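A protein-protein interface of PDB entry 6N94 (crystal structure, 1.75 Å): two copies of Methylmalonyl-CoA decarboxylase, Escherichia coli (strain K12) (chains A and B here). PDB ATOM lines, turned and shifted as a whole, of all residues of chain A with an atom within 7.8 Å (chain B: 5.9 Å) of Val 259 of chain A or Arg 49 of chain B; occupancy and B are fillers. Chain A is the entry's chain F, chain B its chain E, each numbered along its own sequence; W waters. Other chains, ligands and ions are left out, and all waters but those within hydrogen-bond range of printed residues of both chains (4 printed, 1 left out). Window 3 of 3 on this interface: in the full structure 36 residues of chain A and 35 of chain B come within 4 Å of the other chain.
O of Phe 258 of chain A sits at hydrogen-bond distance from NH2 of Arg 49 of chain B (2.9 Å).
Of the 9 printed residues of chain A, 4 touch a printed residue of chain B.
Hydrophobic or aromatic side chains of chain B that line the printed part of chain A: Ala 202 and Pro 203.
No position is printed for both chains.
Water W1 lies within hydrogen-bond range of OD1 of Asn 257 of chain A (2.7 Å), O of Phe 258 of chain A (2.7 Å) and NZ of Lys 13 of chain B (3.0 Å).
Water W4 lies within hydrogen-bond range of OE1 of Glu 200 of chain B and OD1 of Asn 257 of chain A.
Water W2 lies within hydrogen-bond range of NH1 of Arg 49 of chain B, NZ of Lys 13 of chain B, O of Ser 199 of chain B and O of Phe 258 of chain A.
Water W3 bridges the backbone carbonyl oxygen of Glu 200 of chain B (2.9 Å) and the backbone NH of Phe 258 of chain A (3.0 Å).
Of chain B, only Arg 49 (3.7 Å) comes within 4 Å of Val 259 of chain A.
Of the printed residues of chain A, Arg 49 of chain B touches Phe 258 (2.9 Å) and Val 259 (3.7 Å).
Of the printed residues of chain A, Glu 200 of chain B touches Phe 258.
Of the printed residues of chain A, Ala 202 of chain B touches Phe 258 (3.5 Å).
Printed residues of chain A within 4 Å of Pro 203 of chain B: Asp 242, Phe 258 and Gly 260.
Of the printed residues of chain B, Gly 260 of chain A touches Pro 203.
Printed residues of chain A within 4 Å of Lys 201 of chain B: Phe 258 (3.5 Å).
Asp 242 of chain A touches Pro 203 of chain B.
Phe 258 of chain A touches Glu 200 of chain B (CD2 to O, 3.6 Å).
C of Lys 201 of chain B touches CD2 of Phe 258 of chain A, at 3.5 Å.
Phe 258 of chain A touches Ala 202 of chain B (CD2 to N, 3.5 Å).
CB of Phe 258 of chain A touches CD of Pro 203 of chain B, 3.8 Å away.
Val 259 of chain A touches Arg 49 of chain B.
Gly 260 of chain A touches Pro 203 of chain B.
The backbone NH (N) of Val 259 of chain A sits at hydrogen-bond distance from the side-chain carboxylate (OD1) of Asp 242 of chain A (2.9 Å).
O of Lys 13 of chain B sits at hydrogen-bond distance from N of Arg 49 of chain B (2.8 Å).
The side-chain carboxylate (OD2) of Asp 242 of chain A sits at hydrogen-bond distance from the backbone NH (N) of Gly 260 of chain A (2.8 Å).
The chain-end carboxylate (OXT) of His 261 of chain A lies within hydrogen-bond range of the backbone NH (N) of Asp 242 of chain A (2.8 Å).
The backbone carbonyl oxygen (O) of Pro 46 of chain B is in hydrogen-bond range of the guanidinium group (NE) of Arg 49 of chain B, 3.0 Å away.
NZ of Lys 13 of chain B is in salt-bridge range of OE2 of Glu 200 of chain B, 3.3 Å away.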
ATOM      1  N   GLU A 241       0.537 -20.964  -8.327  1.00  0.00           N
ATOM      2  CA  GLU A 241       1.090 -21.696  -7.146  1.00  0.00           C
ATOM      3  C   GLU A 241      -0.020 -22.543  -6.512  1.00  0.00           C
ATOM      4  O   GLU A 241       0.259 -23.680  -6.103  1.00  0.00           O
ATOM      5  CB  GLU A 241       1.646 -20.727  -6.112  1.00  0.00           C
ATOM      6  CG  GLU A 241       2.760 -19.833  -6.651  1.00  0.00           C
ATOM      7  CD  GLU A 241       4.173 -20.389  -6.559  1.00  0.00           C
ATOM      8  OE1 GLU A 241       4.342 -21.527  -6.045  1.00  0.00           O
ATOM      9  OE2 GLU A 241       5.105 -19.669  -7.005  1.00  0.00           O
ATOM     10  N   ASP A 242      -1.237 -21.986  -6.388  1.00  0.00           N
ATOM     11  CA  ASP A 242      -2.376 -22.701  -5.730  1.00  0.00           C
ATOM     12  C   ASP A 242      -2.663 -24.040  -6.388  1.00  0.00           C
ATOM     13  O   ASP A 242      -2.960 -25.016  -5.663  1.00  0.00           O
ATOM     14  CB  ASP A 242      -3.625 -21.820  -5.667  1.00  0.00           C
ATOM     15  CG  ASP A 242      -3.634 -20.798  -4.538  1.00  0.00           C
ATOM     16  OD1 ASP A 242      -2.713 -20.830  -3.681  1.00  0.00           O
ATOM     17  OD2 ASP A 242      -4.556 -19.956  -4.530  1.00  0.00           O
ATOM     18  N   GLU A 245       0.025 -26.500  -5.345  1.00  0.00           N
ATOM     19  CA  GLU A 245      -0.241 -26.779  -3.898  1.00  0.00           C
ATOM     20  C   GLU A 245      -1.452 -27.692  -3.750  1.00  0.00           C
ATOM     21  O   GLU A 245      -1.366 -28.595  -2.930  1.00  0.00           O
ATOM     22  CB  GLU A 245      -0.486 -25.504  -3.115  1.00  0.00           C
ATOM     23  CG  GLU A 245      -1.088 -25.695  -1.736  1.00  0.00           C
ATOM     24  CD  GLU A 245      -0.147 -26.282  -0.674  1.00  0.00           C
ATOM     25  OE1 GLU A 245       1.037 -26.614  -1.030  1.00  0.00           O
ATOM     26  OE2 GLU A 245      -0.631 -26.480   0.481  1.00  0.00           O
ATOM     27  N   PRO A 256      -4.552 -28.463   2.041  1.00  0.00           N
ATOM     28  CA  PRO A 256      -3.847 -27.451   1.256  1.00  0.00           C
ATOM     29  C   PRO A 256      -3.914 -26.085   1.948  1.00  0.00           C
ATOM     30  O   PRO A 256      -4.894 -25.779   2.631  1.00  0.00           O
ATOM     31  CB  PRO A 256      -4.648 -27.418  -0.068  1.00  0.00           C
ATOM     32  CG  PRO A 256      -6.045 -27.840   0.372  1.00  0.00           C
ATOM     33  CD  PRO A 256      -5.769 -28.953   1.354  1.00  0.00           C
ATOM     34  N   ASN A 257      -2.925 -25.252   1.670  1.00  0.00           N
ATOM     35  CA  ASN A 257      -2.936 -23.825   2.072  1.00  0.00           C
ATOM     36  C   ASN A 257      -2.964 -22.941   0.821  1.00  0.00           C
ATOM     37  O   ASN A 257      -1.893 -22.691   0.261  1.00  0.00           O
ATOM     38  CB  ASN A 257      -1.723 -23.467   2.941  1.00  0.00           C
ATOM     39  CG  ASN A 257      -1.902 -22.096   3.561  1.00  0.00           C
ATOM     40  OD1 ASN A 257      -2.909 -21.842   4.227  1.00  0.00           O
ATOM     41  ND2 ASN A 257      -0.966 -21.197   3.314  1.00  0.00           N
ATOM     42  N   PHE A 258      -4.147 -22.464   0.404  1.00  0.00           N
ATOM     43  CA  PHE A 258      -4.319 -21.611  -0.799  1.00  0.00           C
ATOM     44  C   PHE A 258      -4.080 -20.133  -0.421  1.00  0.00           C
ATOM     45  O   PHE A 258      -4.569 -19.686   0.625  1.00  0.00           O
ATOM     46  CB  PHE A 258      -5.710 -21.853  -1.414  1.00  0.00           C
ATOM     47  CG  PHE A 258      -5.940 -23.265  -1.876  1.00  0.00           C
ATOM     48  CD1 PHE A 258      -5.132 -23.828  -2.846  1.00  0.00           C
ATOM     49  CD2 PHE A 258      -6.963 -24.037  -1.341  1.00  0.00           C
ATOM     50  CE1 PHE A 258      -5.327 -25.126  -3.259  1.00  0.00           C
ATOM     51  CE2 PHE A 258      -7.162 -25.322  -1.782  1.00  0.00           C
ATOM     52  CZ  PHE A 258      -6.357 -25.863  -2.751  1.00  0.00           C
ATOM     53  N   VAL A 259      -3.431 -19.367  -1.295  1.00  0.00           N
ATOM     54  CA  VAL A 259      -3.043 -17.953  -1.039  1.00  0.00           C
ATOM     55  C   VAL A 259      -3.544 -16.997  -2.127  1.00  0.00           C
ATOM     56  O   VAL A 259      -3.330 -15.789  -1.993  1.00  0.00           O
ATOM     57  CB  VAL A 259      -1.511 -17.898  -0.892  1.00  0.00           C
ATOM     58  CG1 VAL A 259      -1.037 -18.779   0.252  1.00  0.00           C
ATOM     59  CG2 VAL A 259      -0.802 -18.270  -2.174  1.00  0.00           C
ATOM     60  N   GLY A 260      -4.139 -17.469  -3.213  1.00  0.00           N
ATOM     61  CA  GLY A 260      -4.657 -16.517  -4.214  1.00  0.00           C
ATOM     62  C   GLY A 260      -3.649 -16.154  -5.298  1.00  0.00           C
ATOM     63  O   GLY A 260      -3.915 -15.195  -6.031  1.00  0.00           O
ATOM     64  N   HIS A 261      -2.580 -16.934  -5.503  1.00  0.00           N
ATOM     65  CA  HIS A 261      -1.716 -16.805  -6.711  1.00  0.00           C
ATOM     66  C   HIS A 261      -1.157 -18.171  -7.062  1.00  0.00           C
ATOM     67  O   HIS A 261      -0.306 -18.249  -7.983  1.00  0.00           O
ATOM     68  CB  HIS A 261      -0.628 -15.717  -6.555  1.00  0.00           C
ATOM     69  CG  HIS A 261       0.242 -15.879  -5.345  1.00  0.00           C
ATOM     70  ND1 HIS A 261       1.349 -16.711  -5.319  1.00  0.00           N
ATOM     71  CD2 HIS A 261       0.184 -15.297  -4.128  1.00  0.00           C
ATOM     72  CE1 HIS A 261       1.938 -16.643  -4.138  1.00  0.00           C
ATOM     73  NE2 HIS A 261       1.263 -15.759  -3.400  1.00  0.00           N
ATOM     74  OXT HIS A 261      -1.556 -19.195  -6.436  1.00  0.00           O
ATOM     75  N   LYS B  13     -10.828 -14.222   6.571  1.00  0.00           N
ATOM     76  CA  LYS B  13     -11.013 -14.137   5.103  1.00  0.00           C
ATOM     77  C   LYS B  13     -12.453 -13.739   4.756  1.00  0.00           C
ATOM     78  O   LYS B  13     -12.721 -13.537   3.549  1.00  0.00           O
ATOM     79  CB  LYS B  13     -10.565 -15.491   4.521  1.00  0.00           C
ATOM     80  CG  LYS B  13      -9.083 -15.777   4.623  1.00  0.00           C
ATOM     81  CD  LYS B  13      -8.731 -17.222   4.405  1.00  0.00           C
ATOM     82  CE  LYS B  13      -7.263 -17.521   4.635  1.00  0.00           C
ATOM     83  NZ  LYS B  13      -7.014 -18.990   4.590  1.00  0.00           N
ATOM     84  N   VAL B  14     -13.357 -13.589   5.725  1.00  0.00           N
ATOM     85  CA  VAL B  14     -14.788 -13.262   5.434  1.00  0.00           C
ATOM     86  C   VAL B  14     -15.030 -11.791   5.715  1.00  0.00           C
ATOM     87  O   VAL B  14     -14.666 -11.317   6.810  1.00  0.00           O
ATOM     88  CB  VAL B  14     -15.749 -14.139   6.245  1.00  0.00           C
ATOM     89  CG1 VAL B  14     -17.201 -13.712   6.066  1.00  0.00           C
ATOM     90  CG2 VAL B  14     -15.549 -15.605   5.885  1.00  0.00           C
ATOM     91  N   ARG B  45      -9.403  -7.821  -2.620  1.00  0.00           N
ATOM     92  CA  ARG B  45      -8.025  -8.014  -2.119  1.00  0.00           C
ATOM     93  C   ARG B  45      -7.859  -9.515  -1.967  1.00  0.00           C
ATOM     94  O   ARG B  45      -8.833 -10.181  -1.618  1.00  0.00           O
ATOM     95  CB  ARG B  45      -7.829  -7.358  -0.745  1.00  0.00           C
ATOM     96  CG  ARG B  45      -8.224  -5.893  -0.675  1.00  0.00           C
ATOM     97  CD  ARG B  45      -7.683  -5.242   0.584  1.00  0.00           C
ATOM     98  NE  ARG B  45      -8.135  -5.834   1.854  1.00  0.00           N
ATOM     99  CZ  ARG B  45      -9.176  -5.410   2.581  1.00  0.00           C
ATOM    100  NH1 ARG B  45      -9.916  -4.384   2.191  1.00  0.00           N
ATOM    101  NH2 ARG B  45      -9.438  -5.976   3.742  1.00  0.00           N
ATOM    102  N   PRO B  46      -6.664 -10.061  -2.250  1.00  0.00           N
ATOM    103  CA  PRO B  46      -6.385 -11.507  -2.179  1.00  0.00           C
ATOM    104  C   PRO B  46      -6.699 -12.216  -0.852  1.00  0.00           C
ATOM    105  O   PRO B  46      -7.040 -13.391  -0.895  1.00  0.00           O
ATOM    106  CB  PRO B  46      -4.866 -11.647  -2.393  1.00  0.00           C
ATOM    107  CG  PRO B  46      -4.411 -10.305  -2.910  1.00  0.00           C
ATOM    108  CD  PRO B  46      -5.487  -9.279  -2.646  1.00  0.00           C
ATOM    109  N   GLU B  47      -6.601 -11.486   0.256  1.00  0.00           N
ATOM    110  CA  GLU B  47      -6.770 -12.049   1.613  1.00  0.00           C
ATOM    111  C   GLU B  47      -8.256 -12.047   2.007  1.00  0.00           C
ATOM    112  O   GLU B  47      -8.551 -12.576   3.068  1.00  0.00           O
ATOM    113  CB  GLU B  47      -5.933 -11.304   2.657  1.00  0.00           C
ATOM    114  CG  GLU B  47      -6.353  -9.865   2.932  1.00  0.00           C
ATOM    115  CD  GLU B  47      -5.804  -8.755   2.033  1.00  0.00           C
ATOM    116  OE1 GLU B  47      -5.273  -9.025   0.906  1.00  0.00           O
ATOM    117  OE2 GLU B  47      -5.998  -7.597   2.427  1.00  0.00           O
ATOM    118  N   ILE B  48      -9.140 -11.444   1.205  1.00  0.00           N
ATOM    119  CA  ILE B  48     -10.617 -11.579   1.385  1.00  0.00           C
ATOM    120  C   ILE B  48     -11.112 -12.655   0.422  1.00  0.00           C
ATOM    121  O   ILE B  48     -10.721 -12.591  -0.779  1.00  0.00           O
ATOM    122  CB  ILE B  48     -11.327 -10.259   1.125  1.00  0.00           C
ATOM    123  CG1 ILE B  48     -10.811  -9.161   2.076  1.00  0.00           C
ATOM    124  CG2 ILE B  48     -12.839 -10.456   1.215  1.00  0.00           C
ATOM    125  CD1 ILE B  48     -11.039  -9.462   3.512  1.00  0.00           C
ATOM    126  N   ARG B  49     -11.908 -13.608   0.918  1.00  0.00           N
ATOM    127  CA  ARG B  49     -12.297 -14.798   0.110  1.00  0.00           C
ATOM    128  C   ARG B  49     -13.813 -14.920  -0.075  1.00  0.00           C
ATOM    129  O   ARG B  49     -14.212 -15.651  -0.945  1.00  0.00           O
ATOM    130  CB  ARG B  49     -11.760 -16.052   0.768  1.00  0.00           C
ATOM    131  CG  ARG B  49     -10.242 -16.012   0.902  1.00  0.00           C
ATOM    132  CD  ARG B  49      -9.474 -15.875  -0.391  1.00  0.00           C
ATOM    133  NE  ARG B  49      -8.078 -16.071  -0.041  1.00  0.00           N
ATOM    134  CZ  ARG B  49      -7.517 -17.252   0.206  1.00  0.00           C
ATOM    135  NH1 ARG B  49      -8.215 -18.366   0.074  1.00  0.00           N
ATOM    136  NH2 ARG B  49      -6.260 -17.306   0.609  1.00  0.00           N
ATOM    137  N   CYS B  50     -14.605 -14.293   0.771  1.00  0.00           N
ATOM    138  CA  CYS B  50     -16.077 -14.474   0.758  1.00  0.00           C
ATOM    139  C   CYS B  50     -16.727 -13.229   1.363  1.00  0.00           C
ATOM    140  O   CYS B  50     -16.204 -12.715   2.375  1.00  0.00           O
ATOM    141  CB  CYS B  50     -16.434 -15.757   1.494  1.00  0.00           C
ATOM    142  SG  CYS B  50     -18.135 -16.298   1.221  1.00  0.00           S
ATOM    143  N   ILE B  51     -17.810 -12.764   0.748  1.00  0.00           N
ATOM    144  CA  ILE B  51     -18.570 -11.579   1.182  1.00  0.00           C
ATOM    145  C   ILE B  51     -19.944 -12.026   1.673  1.00  0.00           C
ATOM    146  O   ILE B  51     -20.528 -12.894   1.023  1.00  0.00           O
ATOM    147  CB  ILE B  51     -18.743 -10.574   0.024  1.00  0.00           C
ATOM    148  CG1 ILE B  51     -17.420 -10.257  -0.670  1.00  0.00           C
ATOM    149  CG2 ILE B  51     -19.439  -9.311   0.535  1.00  0.00           C
ATOM    150  CD1 ILE B  51     -16.346  -9.784   0.278  1.00  0.00           C
ATOM    151  N   LYS B  97     -15.192 -13.156  -6.027  1.00  0.00           N
ATOM    152  CA  LYS B  97     -15.353 -13.882  -4.754  1.00  0.00           C
ATOM    153  C   LYS B  97     -16.837 -14.165  -4.603  1.00  0.00           C
ATOM    154  O   LYS B  97     -17.670 -13.413  -5.090  1.00  0.00           O
ATOM    155  CB  LYS B  97     -14.872 -13.016  -3.593  1.00  0.00           C
ATOM    156  CG  LYS B  97     -13.442 -12.493  -3.776  1.00  0.00           C
ATOM    157  CD  LYS B  97     -13.002 -11.629  -2.693  1.00  0.00           C
ATOM    158  CE  LYS B  97     -11.788 -10.804  -3.115  1.00  0.00           C
ATOM    159  NZ  LYS B  97     -10.615 -11.668  -3.339  1.00  0.00           N
ATOM    160  N   PRO B  98     -17.217 -15.251  -3.940  1.00  0.00           N
ATOM    161  CA  PRO B  98     -18.631 -15.506  -3.703  1.00  0.00           C
ATOM    162  C   PRO B  98     -19.233 -14.387  -2.849  1.00  0.00           C
ATOM    163  O   PRO B  98     -18.589 -13.957  -1.888  1.00  0.00           O
ATOM    164  CB  PRO B  98     -18.613 -16.835  -2.939  1.00  0.00           C
ATOM    165  CG  PRO B  98     -17.313 -17.437  -3.306  1.00  0.00           C
ATOM    166  CD  PRO B  98     -16.354 -16.287  -3.401  1.00  0.00           C
ATOM    167  N   ILE B 198     -16.007 -21.965   2.834  1.00  0.00           N
ATOM    168  CA  ILE B 198     -15.690 -21.598   1.421  1.00  0.00           C
ATOM    169  C   ILE B 198     -14.302 -20.943   1.396  1.00  0.00           C
ATOM    170  O   ILE B 198     -13.512 -21.219   0.432  1.00  0.00           O
ATOM    171  CB  ILE B 198     -16.787 -20.675   0.870  1.00  0.00           C
ATOM    172  CG1 ILE B 198     -18.100 -21.425   0.716  1.00  0.00           C
ATOM    173  CG2 ILE B 198     -16.370 -19.976  -0.405  1.00  0.00           C
ATOM    174  CD1 ILE B 198     -19.303 -20.540   0.408  1.00  0.00           C
ATOM    175  N   SER B 199     -13.978 -20.121   2.414  1.00  0.00           N
ATOM    176  CA  SER B 199     -12.724 -19.323   2.440  1.00  0.00           C
ATOM    177  C   SER B 199     -11.493 -20.229   2.550  1.00  0.00           C
ATOM    178  O   SER B 199     -10.410 -19.708   2.294  1.00  0.00           O
ATOM    179  CB  SER B 199     -12.756 -18.260   3.510  1.00  0.00           C
ATOM    180  OG  SER B 199     -13.697 -17.274   3.130  1.00  0.00           O
ATOM    181  N   GLU B 200     -11.662 -21.533   2.830  1.00  0.00           N
ATOM    182  CA  GLU B 200     -10.534 -22.485   2.934  1.00  0.00           C
ATOM    183  C   GLU B 200     -10.220 -23.071   1.558  1.00  0.00           C
ATOM    184  O   GLU B 200      -9.197 -23.738   1.412  1.00  0.00           O
ATOM    185  CB  GLU B 200     -10.846 -23.541   3.994  1.00  0.00           C
ATOM    186  CG  GLU B 200     -10.701 -22.944   5.414  1.00  0.00           C
ATOM    187  CD  GLU B 200      -9.344 -22.247   5.712  1.00  0.00           C
ATOM    188  OE1 GLU B 200      -8.297 -22.996   5.785  1.00  0.00           O
ATOM    189  OE2 GLU B 200      -9.283 -20.949   5.855  1.00  0.00           O
ATOM    190  N   LYS B 201     -11.105 -22.840   0.599  1.00  0.00           N
ATOM    191  CA  LYS B 201     -11.019 -23.475  -0.738  1.00  0.00           C
ATOM    192  C   LYS B 201     -10.160 -22.599  -1.655  1.00  0.00           C
ATOM    193  O   LYS B 201      -9.856 -21.446  -1.304  1.00  0.00           O
ATOM    194  CB  LYS B 201     -12.451 -23.705  -1.254  1.00  0.00           C
ATOM    195  CG  LYS B 201     -13.344 -24.547  -0.333  1.00  0.00           C
ATOM    196  CD  LYS B 201     -12.758 -25.916   0.084  1.00  0.00           C
ATOM    197  CE  LYS B 201     -13.681 -26.716   0.983  1.00  0.00           C
ATOM    198  NZ  LYS B 201     -13.125 -28.056   1.277  1.00  0.00           N
ATOM    199  N   ALA B 202      -9.924 -23.054  -2.876  1.00  0.00           N
ATOM    200  CA  ALA B 202      -8.988 -22.401  -3.817  1.00  0.00           C
ATOM    201  C   ALA B 202      -9.669 -21.209  -4.468  1.00  0.00           C
ATOM    202  O   ALA B 202     -10.601 -21.363  -5.273  1.00  0.00           O
ATOM    203  CB  ALA B 202      -8.498 -23.403  -4.853  1.00  0.00           C
ATOM    204  N   PRO B 203      -9.214 -19.965  -4.167  1.00  0.00           N
ATOM    205  CA  PRO B 203      -9.961 -18.800  -4.631  1.00  0.00           C
ATOM    206  C   PRO B 203      -9.927 -18.598  -6.141  1.00  0.00           C
ATOM    207  O   PRO B 203     -10.852 -18.033  -6.700  1.00  0.00           O
ATOM    208  CB  PRO B 203      -9.298 -17.633  -3.897  1.00  0.00           C
ATOM    209  CG  PRO B 203      -7.884 -18.153  -3.600  1.00  0.00           C
ATOM    210  CD  PRO B 203      -8.104 -19.615  -3.259  1.00  0.00           C
ATOM    211  N   ILE B 206     -12.519 -20.914  -7.607  1.00  0.00           N
ATOM    212  CA  ILE B 206     -13.854 -20.305  -7.334  1.00  0.00           C
ATOM    213  C   ILE B 206     -14.092 -19.167  -8.327  1.00  0.00           C
ATOM    214  O   ILE B 206     -15.167 -19.140  -8.931  1.00  0.00           O
ATOM    215  CB  ILE B 206     -13.950 -19.852  -5.855  1.00  0.00           C
ATOM    216  CG1 ILE B 206     -14.018 -21.095  -4.955  1.00  0.00           C
ATOM    217  CG2 ILE B 206     -15.110 -18.904  -5.658  1.00  0.00           C
ATOM    218  CD1 ILE B 206     -13.822 -20.829  -3.463  1.00  0.00           C
HETATM  219  O   HOH W   1      -4.362 -19.792   3.321  1.00  0.00           O
HETATM  220  O   HOH W   2      -7.616 -20.165   2.080  1.00  0.00           O
HETATM  221  O   HOH W   3      -6.618 -22.682   2.172  1.00  0.00           O
HETATM  222  O   HOH W   4      -5.957 -22.393   4.505  1.00  0.00           O
